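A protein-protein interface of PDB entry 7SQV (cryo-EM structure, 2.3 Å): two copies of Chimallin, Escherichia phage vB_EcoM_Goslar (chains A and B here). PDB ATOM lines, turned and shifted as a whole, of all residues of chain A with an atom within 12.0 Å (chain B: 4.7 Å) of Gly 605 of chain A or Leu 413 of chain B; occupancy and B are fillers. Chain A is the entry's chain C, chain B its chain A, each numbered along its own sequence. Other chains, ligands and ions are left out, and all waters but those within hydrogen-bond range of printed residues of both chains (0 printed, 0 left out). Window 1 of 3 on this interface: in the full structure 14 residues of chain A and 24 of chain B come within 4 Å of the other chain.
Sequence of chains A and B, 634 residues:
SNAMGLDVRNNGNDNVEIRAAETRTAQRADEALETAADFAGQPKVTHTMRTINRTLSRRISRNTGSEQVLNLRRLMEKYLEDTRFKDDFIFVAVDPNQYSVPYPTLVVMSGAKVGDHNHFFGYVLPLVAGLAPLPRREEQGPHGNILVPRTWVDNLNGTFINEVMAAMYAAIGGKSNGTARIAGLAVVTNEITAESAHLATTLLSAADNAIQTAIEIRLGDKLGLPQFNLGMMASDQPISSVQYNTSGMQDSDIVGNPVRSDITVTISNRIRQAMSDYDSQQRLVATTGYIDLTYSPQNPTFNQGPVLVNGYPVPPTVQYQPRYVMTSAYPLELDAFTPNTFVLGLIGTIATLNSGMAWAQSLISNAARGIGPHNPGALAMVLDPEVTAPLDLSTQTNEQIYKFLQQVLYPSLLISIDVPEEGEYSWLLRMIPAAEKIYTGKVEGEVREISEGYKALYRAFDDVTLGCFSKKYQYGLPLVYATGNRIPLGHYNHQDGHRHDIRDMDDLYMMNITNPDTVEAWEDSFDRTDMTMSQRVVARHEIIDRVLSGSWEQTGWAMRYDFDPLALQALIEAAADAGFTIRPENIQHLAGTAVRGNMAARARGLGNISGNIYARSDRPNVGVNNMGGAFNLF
Hydrophobic or aromatic side chains of chain A within 4 Å of the printed part of chain B: Leu 606.
Hydrophobic or aromatic side chains of chain B that line the printed part of chain A: Leu 414 and Pro 565.
No position is printed for both chains.
The backbone NH (N) of Leu 606 of chain A sits at hydrogen-bond distance from the backbone carbonyl oxygen (O) of Leu 413 of chain B, 2.7 Å away.
CD1 of Leu 414 of chain B touches O of Ala 601 of chain A, at 3.5 Å.
Arg 602 of chain A touches Gln 321 of chain B (CA to OE1, 3.9 Å).
O of Arg 604 of chain A touches CG of Leu 414 of chain B, at 3.9 Å.
Pro 565 of chain B touches Arg 604 of chain A.
CA of Gly 605 of chain A touches O of Leu 413 of chain B, 3.5 Å away.
Gly 605 of chain A touches Pro 565 of chain B (O to CB, 3.95 Å).
CD1 of Leu 606 of chain A touches O of Pro 565 of chain B, at 3.9 Å.
NE2 of Gln 321 of chain B is in hydrogen-bond range of OG of Ser 412 of chain B.
O of Pro 322 of chain B sits at hydrogen-bond distance from N of Leu 414 of chain B (3.4 Å).
The backbone NH of Tyr 324 of chain B sits at hydrogen-bond distance from the backbone carbonyl oxygen of Leu 414 of chain B (2.7 Å).
The side-chain sulfur (SD) of Met 599 of chain A lies within hydrogen-bond range of the guanidinium group (NH2) of Arg 602 of chain A (3.3 Å).
Printed residues of chain B within 4 Å of Ala 601 of chain A: Leu 414.
Of the printed residues of chain B, Arg 602 of chain A touches Gln 321.
Printed residues of chain B within 4 Å of Arg 604 of chain A: Leu 414 (3.9 Å) and Pro 565 (3.8 Å).
Gly 605 of chain A touches just these residues of chain B: Leu 413 (3.5 Å) and Pro 565 (3.95 Å).
Of the printed residues of chain B, Leu 606 of chain A touches Leu 413 (2.7 Å) and Pro 565 (3.9 Å).
Of the printed residues of chain A, Gln 321 of chain B touches Arg 602 (3.9 Å).
No residue of chain A comes within 4 Å of Trp 359 of chain B.
Of chain A, only Gly 605 (3.5 Å) and Leu 606 (2.7 Å) come within 4 Å of Leu 413 of chain B.
No residue of chain A comes within 4 Å of Ile 415 of chain B.
Pro 565 of chain B touches just these residues of chain A: Arg 604, Gly 605 and Leu 606.
The nearest residue of chain B that does not touch Gly 605 of chain A is Ser 412 of chain B (4.2 Å).
The nearest residue of chain A that does not touch Leu 413 of chain B is Arg 604 of chain A (4.5 Å).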
ATOM      1  N   ASN A 598      26.539 -39.138  10.576  1.00  0.00           N
ATOM      2  CA  ASN A 598      25.346 -39.332   9.759  1.00  0.00           C
ATOM      3  C   ASN A 598      25.790 -39.600   8.326  1.00  0.00           C
ATOM      4  O   ASN A 598      26.360 -38.720   7.672  1.00  0.00           O
ATOM      5  CB  ASN A 598      24.429 -38.114   9.837  1.00  0.00           C
ATOM      6  CG  ASN A 598      23.080 -38.355   9.190  1.00  0.00           C
ATOM      7  OD1 ASN A 598      22.745 -39.482   8.825  1.00  0.00           O
ATOM      8  ND2 ASN A 598      22.295 -37.294   9.044  1.00  0.00           N
ATOM      9  N   MET A 599      25.529 -40.814   7.841  1.00  0.00           N
ATOM     10  CA  MET A 599      25.964 -41.210   6.507  1.00  0.00           C
ATOM     11  C   MET A 599      25.000 -40.776   5.412  1.00  0.00           C
ATOM     12  O   MET A 599      25.428 -40.570   4.269  1.00  0.00           O
ATOM     13  CB  MET A 599      26.152 -42.728   6.444  1.00  0.00           C
ATOM     14  CG  MET A 599      27.394 -43.232   7.161  1.00  0.00           C
ATOM     15  SD  MET A 599      28.710 -42.001   7.229  1.00  0.00           S
ATOM     16  CE  MET A 599      29.275 -42.201   8.917  1.00  0.00           C
ATOM     17  N   ALA A 600      23.713 -40.632   5.727  1.00  0.00           N
ATOM     18  CA  ALA A 600      22.726 -40.270   4.717  1.00  0.00           C
ATOM     19  C   ALA A 600      22.773 -38.797   4.341  1.00  0.00           C
ATOM     20  O   ALA A 600      22.289 -38.432   3.263  1.00  0.00           O
ATOM     21  CB  ALA A 600      21.320 -40.629   5.203  1.00  0.00           C
ATOM     22  N   ALA A 601      23.338 -37.942   5.196  1.00  0.00           N
ATOM     23  CA  ALA A 601      23.370 -36.513   4.902  1.00  0.00           C
ATOM     24  C   ALA A 601      24.306 -36.193   3.744  1.00  0.00           C
ATOM     25  O   ALA A 601      24.053 -35.245   2.991  1.00  0.00           O
ATOM     26  CB  ALA A 601      23.782 -35.729   6.148  1.00  0.00           C
ATOM     27  N   ARG A 602      25.387 -36.960   3.590  1.00  0.00           N
ATOM     28  CA  ARG A 602      26.350 -36.686   2.529  1.00  0.00           C
ATOM     29  C   ARG A 602      25.736 -36.884   1.148  1.00  0.00           C
ATOM     30  O   ARG A 602      26.022 -36.119   0.221  1.00  0.00           O
ATOM     31  CB  ARG A 602      27.580 -37.576   2.703  1.00  0.00           C
ATOM     32  CG  ARG A 602      28.736 -37.239   1.782  1.00  0.00           C
ATOM     33  CD  ARG A 602      29.857 -38.254   1.928  1.00  0.00           C
ATOM     34  NE  ARG A 602      29.750 -39.004   3.173  1.00  0.00           N
ATOM     35  CZ  ARG A 602      30.289 -40.197   3.380  1.00  0.00           C
ATOM     36  NH1 ARG A 602      30.984 -40.814   2.438  1.00  0.00           N
ATOM     37  NH2 ARG A 602      30.125 -40.788   4.561  1.00  0.00           N
ATOM     38  N   ALA A 603      24.891 -37.903   0.993  1.00  0.00           N
ATOM     39  CA  ALA A 603      24.323 -38.233  -0.308  1.00  0.00           C
ATOM     40  C   ALA A 603      23.197 -37.298  -0.731  1.00  0.00           C
ATOM     41  O   ALA A 603      22.770 -37.360  -1.890  1.00  0.00           O
ATOM     42  CB  ALA A 603      23.812 -39.676  -0.306  1.00  0.00           C
ATOM     43  N   ARG A 604      22.708 -36.441   0.162  1.00  0.00           N
ATOM     44  CA  ARG A 604      21.596 -35.550  -0.139  1.00  0.00           C
ATOM     45  C   ARG A 604      22.045 -34.132  -0.471  1.00  0.00           C
ATOM     46  O   ARG A 604      21.203 -33.232  -0.556  1.00  0.00           O
ATOM     47  CB  ARG A 604      20.610 -35.525   1.029  1.00  0.00           C
ATOM     48  CG  ARG A 604      19.862 -36.832   1.233  1.00  0.00           C
ATOM     49  CD  ARG A 604      18.976 -36.782   2.466  1.00  0.00           C
ATOM     50  NE  ARG A 604      18.521 -38.109   2.859  1.00  0.00           N
ATOM     51  CZ  ARG A 604      17.856 -38.374   3.975  1.00  0.00           C
ATOM     52  NH1 ARG A 604      17.545 -37.420   4.838  1.00  0.00           N
ATOM     53  NH2 ARG A 604      17.491 -39.627   4.232  1.00  0.00           N
ATOM     54  N   GLY A 605      23.343 -33.911  -0.661  1.00  0.00           N
ATOM     55  CA  GLY A 605      23.830 -32.580  -0.985  1.00  0.00           C
ATOM     56  C   GLY A 605      23.602 -32.237  -2.450  1.00  0.00           C
ATOM     57  O   GLY A 605      23.734 -33.078  -3.338  1.00  0.00           O
ATOM     58  N   LEU A 606      23.257 -30.975  -2.693  1.00  0.00           N
ATOM     59  CA  LEU A 606      23.023 -30.465  -4.038  1.00  0.00           C
ATOM     60  C   LEU A 606      24.291 -29.779  -4.531  1.00  0.00           C
ATOM     61  O   LEU A 606      24.716 -28.768  -3.960  1.00  0.00           O
ATOM     62  CB  LEU A 606      21.840 -29.496  -4.056  1.00  0.00           C
ATOM     63  CG  LEU A 606      21.575 -28.760  -5.369  1.00  0.00           C
ATOM     64  CD1 LEU A 606      20.996 -29.708  -6.407  1.00  0.00           C
ATOM     65  CD2 LEU A 606      20.644 -27.580  -5.142  1.00  0.00           C
ATOM     66  N   GLY A 607      24.889 -30.325  -5.586  1.00  0.00           N
ATOM     67  CA  GLY A 607      26.160 -29.825  -6.072  1.00  0.00           C
ATOM     68  C   GLY A 607      26.068 -28.668  -7.046  1.00  0.00           C
ATOM     69  O   GLY A 607      26.633 -27.598  -6.798  1.00  0.00           O
ATOM     70  N   ASN A 608      25.357 -28.863  -8.154  1.00  0.00           N
ATOM     71  CA  ASN A 608      25.287 -27.848  -9.196  1.00  0.00           C
ATOM     72  C   ASN A 608      23.918 -27.891  -9.856  1.00  0.00           C
ATOM     73  O   ASN A 608      23.198 -28.891  -9.778  1.00  0.00           O
ATOM     74  CB  ASN A 608      26.391 -28.041 -10.243  1.00  0.00           C
ATOM     75  CG  ASN A 608      27.430 -26.939 -10.203  1.00  0.00           C
ATOM     76  OD1 ASN A 608      27.405 -26.078  -9.323  1.00  0.00           O
ATOM     77  ND2 ASN A 608      28.354 -26.960 -11.157  1.00  0.00           N
ATOM     78  N   ILE A 609      23.568 -26.786 -10.514  1.00  0.00           N
ATOM     79  CA  ILE A 609      22.298 -26.644 -11.212  1.00  0.00           C
ATOM     80  C   ILE A 609      22.576 -26.207 -12.644  1.00  0.00           C
ATOM     81  O   ILE A 609      23.678 -25.776 -12.987  1.00  0.00           O
ATOM     82  CB  ILE A 609      21.351 -25.645 -10.513  1.00  0.00           C
ATOM     83  CG1 ILE A 609      21.972 -24.249 -10.486  1.00  0.00           C
ATOM     84  CG2 ILE A 609      21.020 -26.117  -9.106  1.00  0.00           C
ATOM     85  CD1 ILE A 609      21.013 -23.163 -10.052  1.00  0.00           C
ATOM     86  N   TYR A 614      19.906 -18.662 -15.713  1.00  0.00           N
ATOM     87  CA  TYR A 614      20.467 -17.328 -15.560  1.00  0.00           C
ATOM     88  C   TYR A 614      20.287 -16.529 -16.843  1.00  0.00           C
ATOM     89  O   TYR A 614      20.358 -17.079 -17.946  1.00  0.00           O
ATOM     90  CB  TYR A 614      21.950 -17.403 -15.191  1.00  0.00           C
ATOM     91  CG  TYR A 614      22.210 -18.097 -13.875  1.00  0.00           C
ATOM     92  CD1 TYR A 614      21.657 -17.617 -12.696  1.00  0.00           C
ATOM     93  CD2 TYR A 614      23.001 -19.236 -13.811  1.00  0.00           C
ATOM     94  CE1 TYR A 614      21.888 -18.249 -11.489  1.00  0.00           C
ATOM     95  CE2 TYR A 614      23.238 -19.875 -12.610  1.00  0.00           C
ATOM     96  CZ  TYR A 614      22.679 -19.377 -11.453  1.00  0.00           C
ATOM     97  OH  TYR A 614      22.911 -20.008 -10.253  1.00  0.00           O
ATOM     98  N   ILE B 291      22.980 -21.123   8.102  1.00  0.00           N
ATOM     99  CA  ILE B 291      23.814 -22.247   7.693  1.00  0.00           C
ATOM    100  C   ILE B 291      24.245 -23.018   8.933  1.00  0.00           C
ATOM    101  O   ILE B 291      24.711 -22.421   9.911  1.00  0.00           O
ATOM    102  CB  ILE B 291      25.042 -21.779   6.891  1.00  0.00           C
ATOM    103  CG1 ILE B 291      24.605 -21.009   5.643  1.00  0.00           C
ATOM    104  CG2 ILE B 291      25.926 -22.962   6.519  1.00  0.00           C
ATOM    105  CD1 ILE B 291      24.194 -21.894   4.486  1.00  0.00           C
ATOM    106  N   GLN B 321      29.568 -31.639   6.599  1.00  0.00           N
ATOM    107  CA  GLN B 321      28.679 -31.343   5.483  1.00  0.00           C
ATOM    108  C   GLN B 321      27.883 -30.079   5.770  1.00  0.00           C
ATOM    109  O   GLN B 321      27.112 -30.048   6.740  1.00  0.00           O
ATOM    110  CB  GLN B 321      27.735 -32.517   5.225  1.00  0.00           C
ATOM    111  CG  GLN B 321      26.559 -32.186   4.321  1.00  0.00           C
ATOM    112  CD  GLN B 321      26.957 -32.076   2.864  1.00  0.00           C
ATOM    113  OE1 GLN B 321      27.528 -33.003   2.293  1.00  0.00           O
ATOM    114  NE2 GLN B 321      26.655 -30.935   2.254  1.00  0.00           N
ATOM    115  N   PRO B 322      28.039 -29.021   4.976  1.00  0.00           N
ATOM    116  CA  PRO B 322      27.232 -27.814   5.188  1.00  0.00           C
ATOM    117  C   PRO B 322      25.754 -28.077   4.943  1.00  0.00           C
ATOM    118  O   PRO B 322      25.372 -28.898   4.106  1.00  0.00           O
ATOM    119  CB  PRO B 322      27.795 -26.822   4.163  1.00  0.00           C
ATOM    120  CG  PRO B 322      29.138 -27.364   3.790  1.00  0.00           C
ATOM    121  CD  PRO B 322      29.017 -28.850   3.891  1.00  0.00           C
ATOM    122  N   ARG B 323      24.917 -27.360   5.691  1.00  0.00           N
ATOM    123  CA  ARG B 323      23.471 -27.508   5.599  1.00  0.00           C
ATOM    124  C   ARG B 323      22.807 -26.144   5.708  1.00  0.00           C
ATOM    125  O   ARG B 323      23.183 -25.327   6.553  1.00  0.00           O
ATOM    126  CB  ARG B 323      22.936 -28.440   6.695  1.00  0.00           C
ATOM    127  CG  ARG B 323      21.425 -28.601   6.694  1.00  0.00           C
ATOM    128  CD  ARG B 323      20.913 -29.015   8.064  1.00  0.00           C
ATOM    129  NE  ARG B 323      21.281 -30.387   8.390  1.00  0.00           N
ATOM    130  CZ  ARG B 323      20.491 -31.437   8.211  1.00  0.00           C
ATOM    131  NH1 ARG B 323      19.272 -31.308   7.712  1.00  0.00           N
ATOM    132  NH2 ARG B 323      20.936 -32.646   8.539  1.00  0.00           N
ATOM    133  N   TYR B 324      21.822 -25.904   4.847  1.00  0.00           N
ATOM    134  CA  TYR B 324      21.043 -24.672   4.851  1.00  0.00           C
ATOM    135  C   TYR B 324      19.656 -24.957   5.411  1.00  0.00           C
ATOM    136  O   TYR B 324      18.986 -25.897   4.971  1.00  0.00           O
ATOM    137  CB  TYR B 324      20.938 -24.083   3.443  1.00  0.00           C
ATOM    138  CG  TYR B 324      19.943 -22.950   3.326  1.00  0.00           C
ATOM    139  CD1 TYR B 324      20.263 -21.671   3.759  1.00  0.00           C
ATOM    140  CD2 TYR B 324      18.684 -23.159   2.777  1.00  0.00           C
ATOM    141  CE1 TYR B 324      19.358 -20.633   3.654  1.00  0.00           C
ATOM    142  CE2 TYR B 324      17.773 -22.128   2.667  1.00  0.00           C
ATOM    143  CZ  TYR B 324      18.114 -20.867   3.107  1.00  0.00           C
ATOM    144  OH  TYR B 324      17.209 -19.838   2.998  1.00  0.00           O
ATOM    145  N   LEU B 353      21.285 -18.910  -4.155  1.00  0.00           N
ATOM    146  CA  LEU B 353      22.278 -19.444  -3.229  1.00  0.00           C
ATOM    147  C   LEU B 353      23.393 -20.210  -3.929  1.00  0.00           C
ATOM    148  O   LEU B 353      24.475 -20.364  -3.352  1.00  0.00           O
ATOM    149  CB  LEU B 353      21.601 -20.350  -2.199  1.00  0.00           C
ATOM    150  CG  LEU B 353      20.918 -19.643  -1.027  1.00  0.00           C
ATOM    151  CD1 LEU B 353      20.417 -20.655  -0.009  1.00  0.00           C
ATOM    152  CD2 LEU B 353      21.862 -18.645  -0.376  1.00  0.00           C
ATOM    153  N   TRP B 359      26.979 -19.105  -0.792  1.00  0.00           N
ATOM    154  CA  TRP B 359      26.618 -19.471   0.573  1.00  0.00           C
ATOM    155  C   TRP B 359      27.813 -19.420   1.516  1.00  0.00           C
ATOM    156  O   TRP B 359      27.639 -19.152   2.711  1.00  0.00           O
ATOM    157  CB  TRP B 359      25.977 -20.862   0.598  1.00  0.00           C
ATOM    158  CG  TRP B 359      26.855 -21.958   0.079  1.00  0.00           C
ATOM    159  CD1 TRP B 359      26.876 -22.462  -1.189  1.00  0.00           C
ATOM    160  CD2 TRP B 359      27.826 -22.704   0.823  1.00  0.00           C
ATOM    161  NE1 TRP B 359      27.807 -23.468  -1.283  1.00  0.00           N
ATOM    162  CE2 TRP B 359      28.403 -23.636  -0.061  1.00  0.00           C
ATOM    163  CE3 TRP B 359      28.266 -22.672   2.150  1.00  0.00           C
ATOM    164  CZ2 TRP B 359      29.397 -24.527   0.338  1.00  0.00           C
ATOM    165  CZ3 TRP B 359      29.253 -23.555   2.544  1.00  0.00           C
ATOM    166  CH2 TRP B 359      29.808 -24.471   1.641  1.00  0.00           C
ATOM    167  N   SER B 412      29.314 -28.875  -1.225  1.00  0.00           N
ATOM    168  CA  SER B 412      27.911 -29.061  -1.569  1.00  0.00           C
ATOM    169  C   SER B 412      27.060 -28.476  -0.454  1.00  0.00           C
ATOM    170  O   SER B 412      27.549 -28.176   0.638  1.00  0.00           O
ATOM    171  CB  SER B 412      27.582 -30.540  -1.801  1.00  0.00           C
ATOM    172  OG  SER B 412      27.761 -31.295  -0.617  1.00  0.00           O
ATOM    173  N   LEU B 413      25.770 -28.314  -0.742  1.00  0.00           N
ATOM    174  CA  LEU B 413      24.826 -27.725   0.196  1.00  0.00           C
ATOM    175  C   LEU B 413      23.604 -28.620   0.338  1.00  0.00           C
ATOM    176  O   LEU B 413      23.121 -29.190  -0.645  1.00  0.00           O
ATOM    177  CB  LEU B 413      24.395 -26.325  -0.255  1.00  0.00           C
ATOM    178  CG  LEU B 413      23.862 -25.390   0.833  1.00  0.00           C
ATOM    179  CD1 LEU B 413      24.883 -25.224   1.947  1.00  0.00           C
ATOM    180  CD2 LEU B 413      23.490 -24.041   0.241  1.00  0.00           C
ATOM    181  N   LEU B 414      23.111 -28.739   1.567  1.00  0.00           N
ATOM    182  CA  LEU B 414      21.900 -29.489   1.866  1.00  0.00           C
ATOM    183  C   LEU B 414      20.770 -28.511   2.159  1.00  0.00           C
ATOM    184  O   LEU B 414      20.943 -27.579   2.953  1.00  0.00           O
ATOM    185  CB  LEU B 414      22.119 -30.426   3.057  1.00  0.00           C
ATOM    186  CG  LEU B 414      21.429 -31.794   3.043  1.00  0.00           C
ATOM    187  CD1 LEU B 414      21.968 -32.664   4.167  1.00  0.00           C
ATOM    188  CD2 LEU B 414      19.919 -31.660   3.153  1.00  0.00           C
ATOM    189  N   ILE B 415      19.623 -28.722   1.523  1.00  0.00           N
ATOM    190  CA  ILE B 415      18.475 -27.832   1.653  1.00  0.00           C
ATOM    191  C   ILE B 415      17.502 -28.442   2.651  1.00  0.00           C
ATOM    192  O   ILE B 415      17.017 -29.563   2.457  1.00  0.00           O
ATOM    193  CB  ILE B 415      17.794 -27.592   0.297  1.00  0.00           C
ATOM    194  CG1 ILE B 415      18.842 -27.338  -0.789  1.00  0.00           C
ATOM    195  CG2 ILE B 415      16.823 -26.425   0.388  1.00  0.00           C
ATOM    196  CD1 ILE B 415      19.612 -26.047  -0.605  1.00  0.00           C
ATOM    197  N   PRO B 565      17.759 -33.762  -3.791  1.00  0.00           N
ATOM    198  CA  PRO B 565      18.497 -32.935  -4.763  1.00  0.00           C
ATOM    199  C   PRO B 565      18.105 -33.187  -6.208  1.00  0.00           C
ATOM    200  O   PRO B 565      18.092 -32.247  -7.015  1.00  0.00           O
ATOM    201  CB  PRO B 565      19.962 -33.311  -4.496  1.00  0.00           C
ATOM    202  CG  PRO B 565      19.903 -34.654  -3.845  1.00  0.00           C
ATOM    203  CD  PRO B 565      18.644 -34.665  -3.036  1.00  0.00           C
